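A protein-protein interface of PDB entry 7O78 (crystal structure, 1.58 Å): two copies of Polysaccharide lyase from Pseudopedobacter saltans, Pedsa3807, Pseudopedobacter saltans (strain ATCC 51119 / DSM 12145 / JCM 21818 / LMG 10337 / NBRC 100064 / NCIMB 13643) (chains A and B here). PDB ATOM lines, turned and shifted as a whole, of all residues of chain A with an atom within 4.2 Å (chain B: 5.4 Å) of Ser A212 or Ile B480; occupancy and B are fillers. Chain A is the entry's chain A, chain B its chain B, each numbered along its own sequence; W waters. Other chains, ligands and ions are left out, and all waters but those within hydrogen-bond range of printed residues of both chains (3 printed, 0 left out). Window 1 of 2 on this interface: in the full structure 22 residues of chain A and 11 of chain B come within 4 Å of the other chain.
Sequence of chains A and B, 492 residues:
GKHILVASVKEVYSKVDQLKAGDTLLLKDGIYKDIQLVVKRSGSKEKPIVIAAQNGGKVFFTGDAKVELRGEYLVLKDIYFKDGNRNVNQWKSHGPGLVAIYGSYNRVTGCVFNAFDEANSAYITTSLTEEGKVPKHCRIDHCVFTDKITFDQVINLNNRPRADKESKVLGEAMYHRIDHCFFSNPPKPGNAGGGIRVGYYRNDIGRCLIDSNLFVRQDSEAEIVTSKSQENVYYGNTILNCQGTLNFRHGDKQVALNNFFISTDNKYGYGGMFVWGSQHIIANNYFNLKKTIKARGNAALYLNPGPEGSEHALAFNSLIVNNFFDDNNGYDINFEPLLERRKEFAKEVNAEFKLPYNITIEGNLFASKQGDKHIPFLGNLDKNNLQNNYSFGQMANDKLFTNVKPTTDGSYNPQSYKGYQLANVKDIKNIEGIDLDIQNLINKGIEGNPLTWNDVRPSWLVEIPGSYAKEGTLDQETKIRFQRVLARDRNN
No position is printed for both chains. Of the 9 pairs that touch across the chains among the printed residues, none has its exchanged pair printed and touching as well.
Gln B476 touches Arg A177. NH2 of Arg A177 touches CG1 of Ile B480, at 3.5 Å. Asp A211 touches Ile B480. Ser A212 touches Ile B480 (OG to CG2, 3.5 Å). Glu B477 touches Tyr A235. CE2 of Tyr A235 touches CD1 of Ile B480, at 3.7 Å. Leu A451 touches Arg B484.
Printed residues of chain A that touch a printed residue of chain B: Arg A177, His A180, Asp A211, Ser A212, Tyr A235 and Leu A451. Hydrophobic or aromatic side chains of chain A within 4 Å of the printed part of chain B: His A180, Tyr A235 and Leu A451. Printed residues of chain B that touch a printed residue of chain A: Gln B476, Glu B477, Ile B480, Gln B483 and Arg B484. Hydrophobic or aromatic side chains of chain B within 4 Å of the printed part of chain A: Ile B480. Along chain B the printed residues that touch a printed residue of chain A span positions 476 to 484. Among the printed residues, 9 pairs touch across the chains.
Water W2 bridges NE2 of His A180 (2.7 Å) and O of Ile B480 (3.0 Å). Water W1 bridges the side-chain carboxylate of Glu B477 (3.0 Å) and the side-chain hydroxyl of Tyr A235 (3.4 Å). Water W3 bridges NH1 of Arg A177 (3.1 Å) and NE2 of Gln B483 (3.5 Å).
Of the printed residues of chain B, His A180 touches Gln B483 (3.2 Å). Of the printed residues of chain B, Asp A211 touches Ile B480. Of chain B, only Ile B480 comes within 4 Å of Ser A212. Of the printed residues of chain B, Tyr A235 touches Glu B477 and Ile B480. The nearest printed residue of chain B that does not touch Arg A177 is Lys B479 (4.8 Å).
NH2 of Arg A177 is in hydrogen-bond range of OE1 of Gln B483 (3.1 Å). ND1 of His A180 lies close to NE2 of Gln B483, 3.5 Å away.
O of Asp A211 lies within hydrogen-bond range of N of His A180, 3.4 Å away. OD2 of Asp A211 lies within hydrogen-bond range of OG of Ser A212 (2.7 Å). O of Lys B479 sits close to OE1 of Gln B483 (3.2 Å). ND2 of Asn A237 sits close to N of Tyr A235 (3.4 Å). The backbone NH of Ser A212 is in hydrogen-bond range of the side-chain amide oxygen of Asn A237, 3.4 Å away. The backbone NH (N) of His A180 sits at hydrogen-bond distance from the backbone carbonyl oxygen (O) of Ser A212 (3.0 Å).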
ATOM      1  N   ARG A 177     -23.597 -40.080  -3.701  1.00  0.00           N
ATOM      2  CA  ARG A 177     -23.138 -38.702  -3.423  1.00  0.00           C
ATOM      3  C   ARG A 177     -21.670 -38.776  -3.050  1.00  0.00           C
ATOM      4  O   ARG A 177     -21.286 -39.603  -2.228  1.00  0.00           O
ATOM      5  CB  ARG A 177     -23.932 -38.051  -2.286  1.00  0.00           C
ATOM      6  CG  ARG A 177     -23.519 -36.592  -2.063  1.00  0.00           C
ATOM      7  CD  ARG A 177     -24.402 -35.951  -0.966  1.00  0.00           C
ATOM      8  NE  ARG A 177     -23.937 -34.570  -0.765  1.00  0.00           N
ATOM      9  CZ  ARG A 177     -23.982 -33.914   0.415  1.00  0.00           C
ATOM     10  NH1 ARG A 177     -24.474 -34.501   1.528  1.00  0.00           N
ATOM     11  NH2 ARG A 177     -23.478 -32.686   0.496  1.00  0.00           N
ATOM     12  N   HIS A 180     -17.568 -33.044  -0.137  1.00  0.00           N
ATOM     13  CA  HIS A 180     -16.587 -32.573   0.858  1.00  0.00           C
ATOM     14  C   HIS A 180     -15.338 -33.454   0.861  1.00  0.00           C
ATOM     15  O   HIS A 180     -14.764 -33.759   1.900  1.00  0.00           O
ATOM     16  CB  HIS A 180     -17.241 -32.518   2.250  1.00  0.00           C
ATOM     17  CG  HIS A 180     -18.364 -31.551   2.278  1.00  0.00           C
ATOM     18  ND1 HIS A 180     -19.682 -31.918   2.035  1.00  0.00           N
ATOM     19  CD2 HIS A 180     -18.358 -30.206   2.441  1.00  0.00           C
ATOM     20  CE1 HIS A 180     -20.446 -30.819   2.077  1.00  0.00           C
ATOM     21  NE2 HIS A 180     -19.670 -29.773   2.323  1.00  0.00           N
ATOM     22  N   CYS A 181     -14.902 -33.884  -0.315  1.00  0.00           N
ATOM     23  CA  CYS A 181     -13.686 -34.668  -0.395  1.00  0.00           C
ATOM     24  C   CYS A 181     -12.559 -33.813  -0.955  1.00  0.00           C
ATOM     25  O   CYS A 181     -12.804 -32.817  -1.622  1.00  0.00           O
ATOM     26  CB  CYS A 181     -13.877 -35.918  -1.302  1.00  0.00           C
ATOM     27  SG  CYS A 181     -14.878 -37.193  -0.472  1.00  0.00           S
ATOM     28  N   ASP A 211     -20.603 -33.021  -5.217  1.00  0.00           N
ATOM     29  CA  ASP A 211     -20.782 -31.651  -4.741  1.00  0.00           C
ATOM     30  C   ASP A 211     -19.754 -31.287  -3.677  1.00  0.00           C
ATOM     31  O   ASP A 211     -19.328 -32.115  -2.899  1.00  0.00           O
ATOM     32  CB  ASP A 211     -22.221 -31.411  -4.201  1.00  0.00           C
ATOM     33  CG  ASP A 211     -22.471 -32.051  -2.863  1.00  0.00           C
ATOM     34  OD1 ASP A 211     -22.869 -33.230  -2.844  1.00  0.00           O
ATOM     35  OD2 ASP A 211     -22.200 -31.429  -1.802  1.00  0.00           O
ATOM     36  N   SER A 212     -19.443 -30.008  -3.615  1.00  0.00           N
ATOM     37  CA  SER A 212     -18.665 -29.462  -2.487  1.00  0.00           C
ATOM     38  C   SER A 212     -17.321 -30.153  -2.338  1.00  0.00           C
ATOM     39  O   SER A 212     -16.830 -30.311  -1.212  1.00  0.00           O
ATOM     40  CB  SER A 212     -19.416 -29.596  -1.153  1.00  0.00           C
ATOM     41  OG  SER A 212     -20.778 -29.128  -1.314  1.00  0.00           O
ATOM     42  N   ASN A 213     -16.692 -30.570  -3.435  1.00  0.00           N
ATOM     43  CA  ASN A 213     -15.384 -31.188  -3.333  1.00  0.00           C
ATOM     44  C   ASN A 213     -14.303 -30.183  -3.721  1.00  0.00           C
ATOM     45  O   ASN A 213     -14.539 -29.245  -4.462  1.00  0.00           O
ATOM     46  CB  ASN A 213     -15.312 -32.412  -4.274  1.00  0.00           C
ATOM     47  CG  ASN A 213     -16.312 -33.466  -3.873  1.00  0.00           C
ATOM     48  OD1 ASN A 213     -16.137 -34.128  -2.829  1.00  0.00           O
ATOM     49  ND2 ASN A 213     -17.353 -33.649  -4.695  1.00  0.00           N
ATOM     50  N   TYR A 235     -22.029 -29.984  -8.587  1.00  0.00           N
ATOM     51  CA  TYR A 235     -22.482 -28.759  -7.942  1.00  0.00           C
ATOM     52  C   TYR A 235     -21.504 -28.231  -6.892  1.00  0.00           C
ATOM     53  O   TYR A 235     -21.175 -28.933  -5.941  1.00  0.00           O
ATOM     54  CB  TYR A 235     -23.815 -29.097  -7.267  1.00  0.00           C
ATOM     55  CG  TYR A 235     -24.471 -27.960  -6.508  1.00  0.00           C
ATOM     56  CD1 TYR A 235     -24.761 -26.745  -7.102  1.00  0.00           C
ATOM     57  CD2 TYR A 235     -24.901 -28.170  -5.230  1.00  0.00           C
ATOM     58  CE1 TYR A 235     -25.397 -25.696  -6.369  1.00  0.00           C
ATOM     59  CE2 TYR A 235     -25.566 -27.137  -4.499  1.00  0.00           C
ATOM     60  CZ  TYR A 235     -25.798 -25.931  -5.089  1.00  0.00           C
ATOM     61  OH  TYR A 235     -26.399 -24.935  -4.323  1.00  0.00           O
ATOM     62  N   GLY A 236     -21.105 -26.977  -7.045  1.00  0.00           N
ATOM     63  CA  GLY A 236     -20.374 -26.318  -5.970  1.00  0.00           C
ATOM     64  C   GLY A 236     -19.012 -26.909  -5.639  1.00  0.00           C
ATOM     65  O   GLY A 236     -18.616 -26.869  -4.463  1.00  0.00           O
ATOM     66  N   ASN A 237     -18.278 -27.429  -6.643  1.00  0.00           N
ATOM     67  CA  ASN A 237     -16.937 -27.967  -6.446  1.00  0.00           C
ATOM     68  C   ASN A 237     -15.942 -26.878  -6.764  1.00  0.00           C
ATOM     69  O   ASN A 237     -16.217 -26.008  -7.582  1.00  0.00           O
ATOM     70  CB  ASN A 237     -16.705 -29.118  -7.412  1.00  0.00           C
ATOM     71  CG  ASN A 237     -17.651 -30.220  -7.188  1.00  0.00           C
ATOM     72  OD1 ASN A 237     -17.519 -30.980  -6.253  1.00  0.00           O
ATOM     73  ND2 ASN A 237     -18.660 -30.340  -8.078  1.00  0.00           N
ATOM     74  N   LEU A 451     -14.214 -23.065  -2.191  1.00  0.00           N
ATOM     75  CA  LEU A 451     -13.933 -23.832  -0.985  1.00  0.00           C
ATOM     76  C   LEU A 451     -12.436 -23.745  -0.629  1.00  0.00           C
ATOM     77  O   LEU A 451     -11.555 -23.615  -1.498  1.00  0.00           O
ATOM     78  CB  LEU A 451     -14.244 -25.326  -1.239  1.00  0.00           C
ATOM     79  CG  LEU A 451     -15.722 -25.582  -1.450  1.00  0.00           C
ATOM     80  CD1 LEU A 451     -15.824 -26.980  -2.138  1.00  0.00           C
ATOM     81  CD2 LEU A 451     -16.418 -25.596  -0.126  1.00  0.00           C
ATOM     82  N   VAL A 456     -13.662 -28.608   3.875  1.00  0.00           N
ATOM     83  CA  VAL A 456     -13.928 -29.994   3.479  1.00  0.00           C
ATOM     84  C   VAL A 456     -13.286 -31.014   4.407  1.00  0.00           C
ATOM     85  O   VAL A 456     -13.685 -32.181   4.379  1.00  0.00           O
ATOM     86  CB  VAL A 456     -13.509 -30.277   2.014  1.00  0.00           C
ATOM     87  CG1 VAL A 456     -14.219 -29.285   1.059  1.00  0.00           C
ATOM     88  CG2 VAL A 456     -11.973 -30.127   1.844  1.00  0.00           C
ATOM     89  N   ASP B 475     -33.315 -30.429   3.120  1.00  0.00           N
ATOM     90  CA  ASP B 475     -33.219 -30.678   1.682  1.00  0.00           C
ATOM     91  C   ASP B 475     -31.758 -30.527   1.272  1.00  0.00           C
ATOM     92  O   ASP B 475     -30.927 -30.040   2.032  1.00  0.00           O
ATOM     93  CB  ASP B 475     -34.101 -29.760   0.834  1.00  0.00           C
ATOM     94  CG  ASP B 475     -33.756 -28.295   0.947  1.00  0.00           C
ATOM     95  OD1 ASP B 475     -32.700 -27.847   0.514  1.00  0.00           O
ATOM     96  OD2 ASP B 475     -34.587 -27.508   1.457  1.00  0.00           O
ATOM     97  N   GLN B 476     -31.428 -31.040   0.083  1.00  0.00           N
ATOM     98  CA  GLN B 476     -30.019 -31.186  -0.256  1.00  0.00           C
ATOM     99  C   GLN B 476     -29.254 -29.858  -0.260  1.00  0.00           C
ATOM    100  O   GLN B 476     -28.119 -29.810   0.237  1.00  0.00           O
ATOM    101  CB  GLN B 476     -29.914 -31.895  -1.604  1.00  0.00           C
ATOM    102  CG  GLN B 476     -28.458 -32.196  -1.992  1.00  0.00           C
ATOM    103  CD  GLN B 476     -27.811 -33.154  -1.044  1.00  0.00           C
ATOM    104  OE1 GLN B 476     -27.070 -32.773  -0.105  1.00  0.00           O
ATOM    105  NE2 GLN B 476     -28.078 -34.397  -1.255  1.00  0.00           N
ATOM    106  N   GLU B 477     -29.799 -28.822  -0.906  1.00  0.00           N
ATOM    107  CA  GLU B 477     -29.119 -27.523  -0.955  1.00  0.00           C
ATOM    108  C   GLU B 477     -28.887 -26.989   0.457  1.00  0.00           C
ATOM    109  O   GLU B 477     -27.783 -26.531   0.799  1.00  0.00           O
ATOM    110  CB  GLU B 477     -29.964 -26.530  -1.787  1.00  0.00           C
ATOM    111  CG  GLU B 477     -29.329 -25.141  -1.857  1.00  0.00           C
ATOM    112  CD  GLU B 477     -30.255 -24.098  -2.485  1.00  0.00           C
ATOM    113  OE1 GLU B 477     -31.295 -24.484  -3.085  1.00  0.00           O
ATOM    114  OE2 GLU B 477     -29.871 -22.925  -2.454  1.00  0.00           O
ATOM    115  N   THR B 478     -29.924 -27.062   1.307  1.00  0.00           N
ATOM    116  CA  THR B 478     -29.801 -26.575   2.681  1.00  0.00           C
ATOM    117  C   THR B 478     -28.761 -27.363   3.470  1.00  0.00           C
ATOM    118  O   THR B 478     -28.003 -26.778   4.267  1.00  0.00           O
ATOM    119  CB  THR B 478     -31.181 -26.632   3.353  1.00  0.00           C
ATOM    120  OG1 THR B 478     -32.019 -25.728   2.615  1.00  0.00           O
ATOM    121  CG2 THR B 478     -31.130 -26.225   4.798  1.00  0.00           C
ATOM    122  N   LYS B 479     -28.661 -28.693   3.233  1.00  0.00           N
ATOM    123  CA  LYS B 479     -27.656 -29.473   3.901  1.00  0.00           C
ATOM    124  C   LYS B 479     -26.260 -28.955   3.549  1.00  0.00           C
ATOM    125  O   LYS B 479     -25.376 -28.915   4.388  1.00  0.00           O
ATOM    126  CB  LYS B 479     -27.746 -30.951   3.460  1.00  0.00           C
ATOM    127  CG  LYS B 479     -28.843 -31.775   4.100  1.00  0.00           C
ATOM    128  CD  LYS B 479     -28.460 -33.259   3.876  1.00  0.00           C
ATOM    129  CE  LYS B 479     -29.490 -34.238   4.422  1.00  0.00           C
ATOM    130  NZ  LYS B 479     -29.730 -35.270   3.381  1.00  0.00           N
ATOM    131  N   ILE B 480     -26.024 -28.677   2.258  1.00  0.00           N
ATOM    132  CA  ILE B 480     -24.725 -28.165   1.844  1.00  0.00           C
ATOM    133  C   ILE B 480     -24.409 -26.802   2.485  1.00  0.00           C
ATOM    134  O   ILE B 480     -23.303 -26.600   2.982  1.00  0.00           O
ATOM    135  CB  ILE B 480     -24.662 -28.108   0.314  1.00  0.00           C
ATOM    136  CG1 ILE B 480     -24.678 -29.535  -0.246  1.00  0.00           C
ATOM    137  CG2 ILE B 480     -23.453 -27.257  -0.164  1.00  0.00           C
ATOM    138  CD1 ILE B 480     -24.980 -29.513  -1.726  1.00  0.00           C
ATOM    139  N   ARG B 481     -25.400 -25.888   2.523  1.00  0.00           N
ATOM    140  CA  ARG B 481     -25.188 -24.587   3.149  1.00  0.00           C
ATOM    141  C   ARG B 481     -24.936 -24.764   4.652  1.00  0.00           C
ATOM    142  O   ARG B 481     -24.070 -24.092   5.233  1.00  0.00           O
ATOM    143  CB  ARG B 481     -26.428 -23.709   2.868  1.00  0.00           C
ATOM    144  CG  ARG B 481     -26.599 -23.456   1.372  1.00  0.00           C
ATOM    145  CD  ARG B 481     -27.537 -22.330   1.088  1.00  0.00           C
ATOM    146  NE  ARG B 481     -26.904 -21.021   1.363  1.00  0.00           N
ATOM    147  CZ  ARG B 481     -27.614 -19.877   1.379  1.00  0.00           C
ATOM    148  NH1 ARG B 481     -28.911 -19.887   1.146  1.00  0.00           N
ATOM    149  NH2 ARG B 481     -26.989 -18.741   1.599  1.00  0.00           N
ATOM    150  N   PHE B 482     -25.650 -25.718   5.280  1.00  0.00           N
ATOM    151  CA  PHE B 482     -25.468 -25.973   6.720  1.00  0.00           C
ATOM    152  C   PHE B 482     -24.056 -26.476   7.000  1.00  0.00           C
ATOM    153  O   PHE B 482     -23.394 -25.998   7.931  1.00  0.00           O
ATOM    154  CB  PHE B 482     -26.549 -26.959   7.187  1.00  0.00           C
ATOM    155  CG  PHE B 482     -26.697 -27.164   8.700  1.00  0.00           C
ATOM    156  CD1 PHE B 482     -26.310 -26.197   9.626  1.00  0.00           C
ATOM    157  CD2 PHE B 482     -27.359 -28.313   9.144  1.00  0.00           C
ATOM    158  CE1 PHE B 482     -26.555 -26.381  10.997  1.00  0.00           C
ATOM    159  CE2 PHE B 482     -27.579 -28.538  10.496  1.00  0.00           C
ATOM    160  CZ  PHE B 482     -27.161 -27.566  11.443  1.00  0.00           C
ATOM    161  N   GLN B 483     -23.535 -27.367   6.133  1.00  0.00           N
ATOM    162  CA  GLN B 483     -22.166 -27.830   6.338  1.00  0.00           C
ATOM    163  C   GLN B 483     -21.162 -26.674   6.226  1.00  0.00           C
ATOM    164  O   GLN B 483     -20.187 -26.652   6.996  1.00  0.00           O
ATOM    165  CB  GLN B 483     -21.862 -28.992   5.327  1.00  0.00           C
ATOM    166  CG  GLN B 483     -22.924 -30.129   5.328  1.00  0.00           C
ATOM    167  CD  GLN B 483     -22.794 -31.242   4.249  1.00  0.00           C
ATOM    168  OE1 GLN B 483     -23.433 -31.170   3.172  1.00  0.00           O
ATOM    169  NE2 GLN B 483     -22.027 -32.307   4.564  1.00  0.00           N
ATOM    170  N   ARG B 484     -21.439 -25.635   5.370  1.00  0.00           N
ATOM    171  CA  ARG B 484     -20.566 -24.451   5.328  1.00  0.00           C
ATOM    172  C   ARG B 484     -20.600 -23.678   6.649  1.00  0.00           C
ATOM    173  O   ARG B 484     -19.563 -23.211   7.140  1.00  0.00           O
ATOM    174  CB  ARG B 484     -20.964 -23.476   4.197  1.00  0.00           C
ATOM    175  CG  ARG B 484     -20.538 -23.783   2.799  1.00  0.00           C
ATOM    176  CD  ARG B 484     -18.968 -23.929   2.625  1.00  0.00           C
ATOM    177  NE  ARG B 484     -18.171 -22.795   2.103  1.00  0.00           N
ATOM    178  CZ  ARG B 484     -18.058 -22.461   0.810  1.00  0.00           C
ATOM    179  NH1 ARG B 484     -18.680 -23.161  -0.136  1.00  0.00           N
ATOM    180  NH2 ARG B 484     -17.293 -21.431   0.439  1.00  0.00           N
HETATM  181  O   HOH W   1     -27.088 -21.954  -2.787  1.00  0.00           O
HETATM  182  O   HOH W   2     -20.464 -27.152   2.312  1.00  0.00           O
HETATM  183  O   HOH W   3     -25.071 -33.964   4.499  1.00  0.00           O
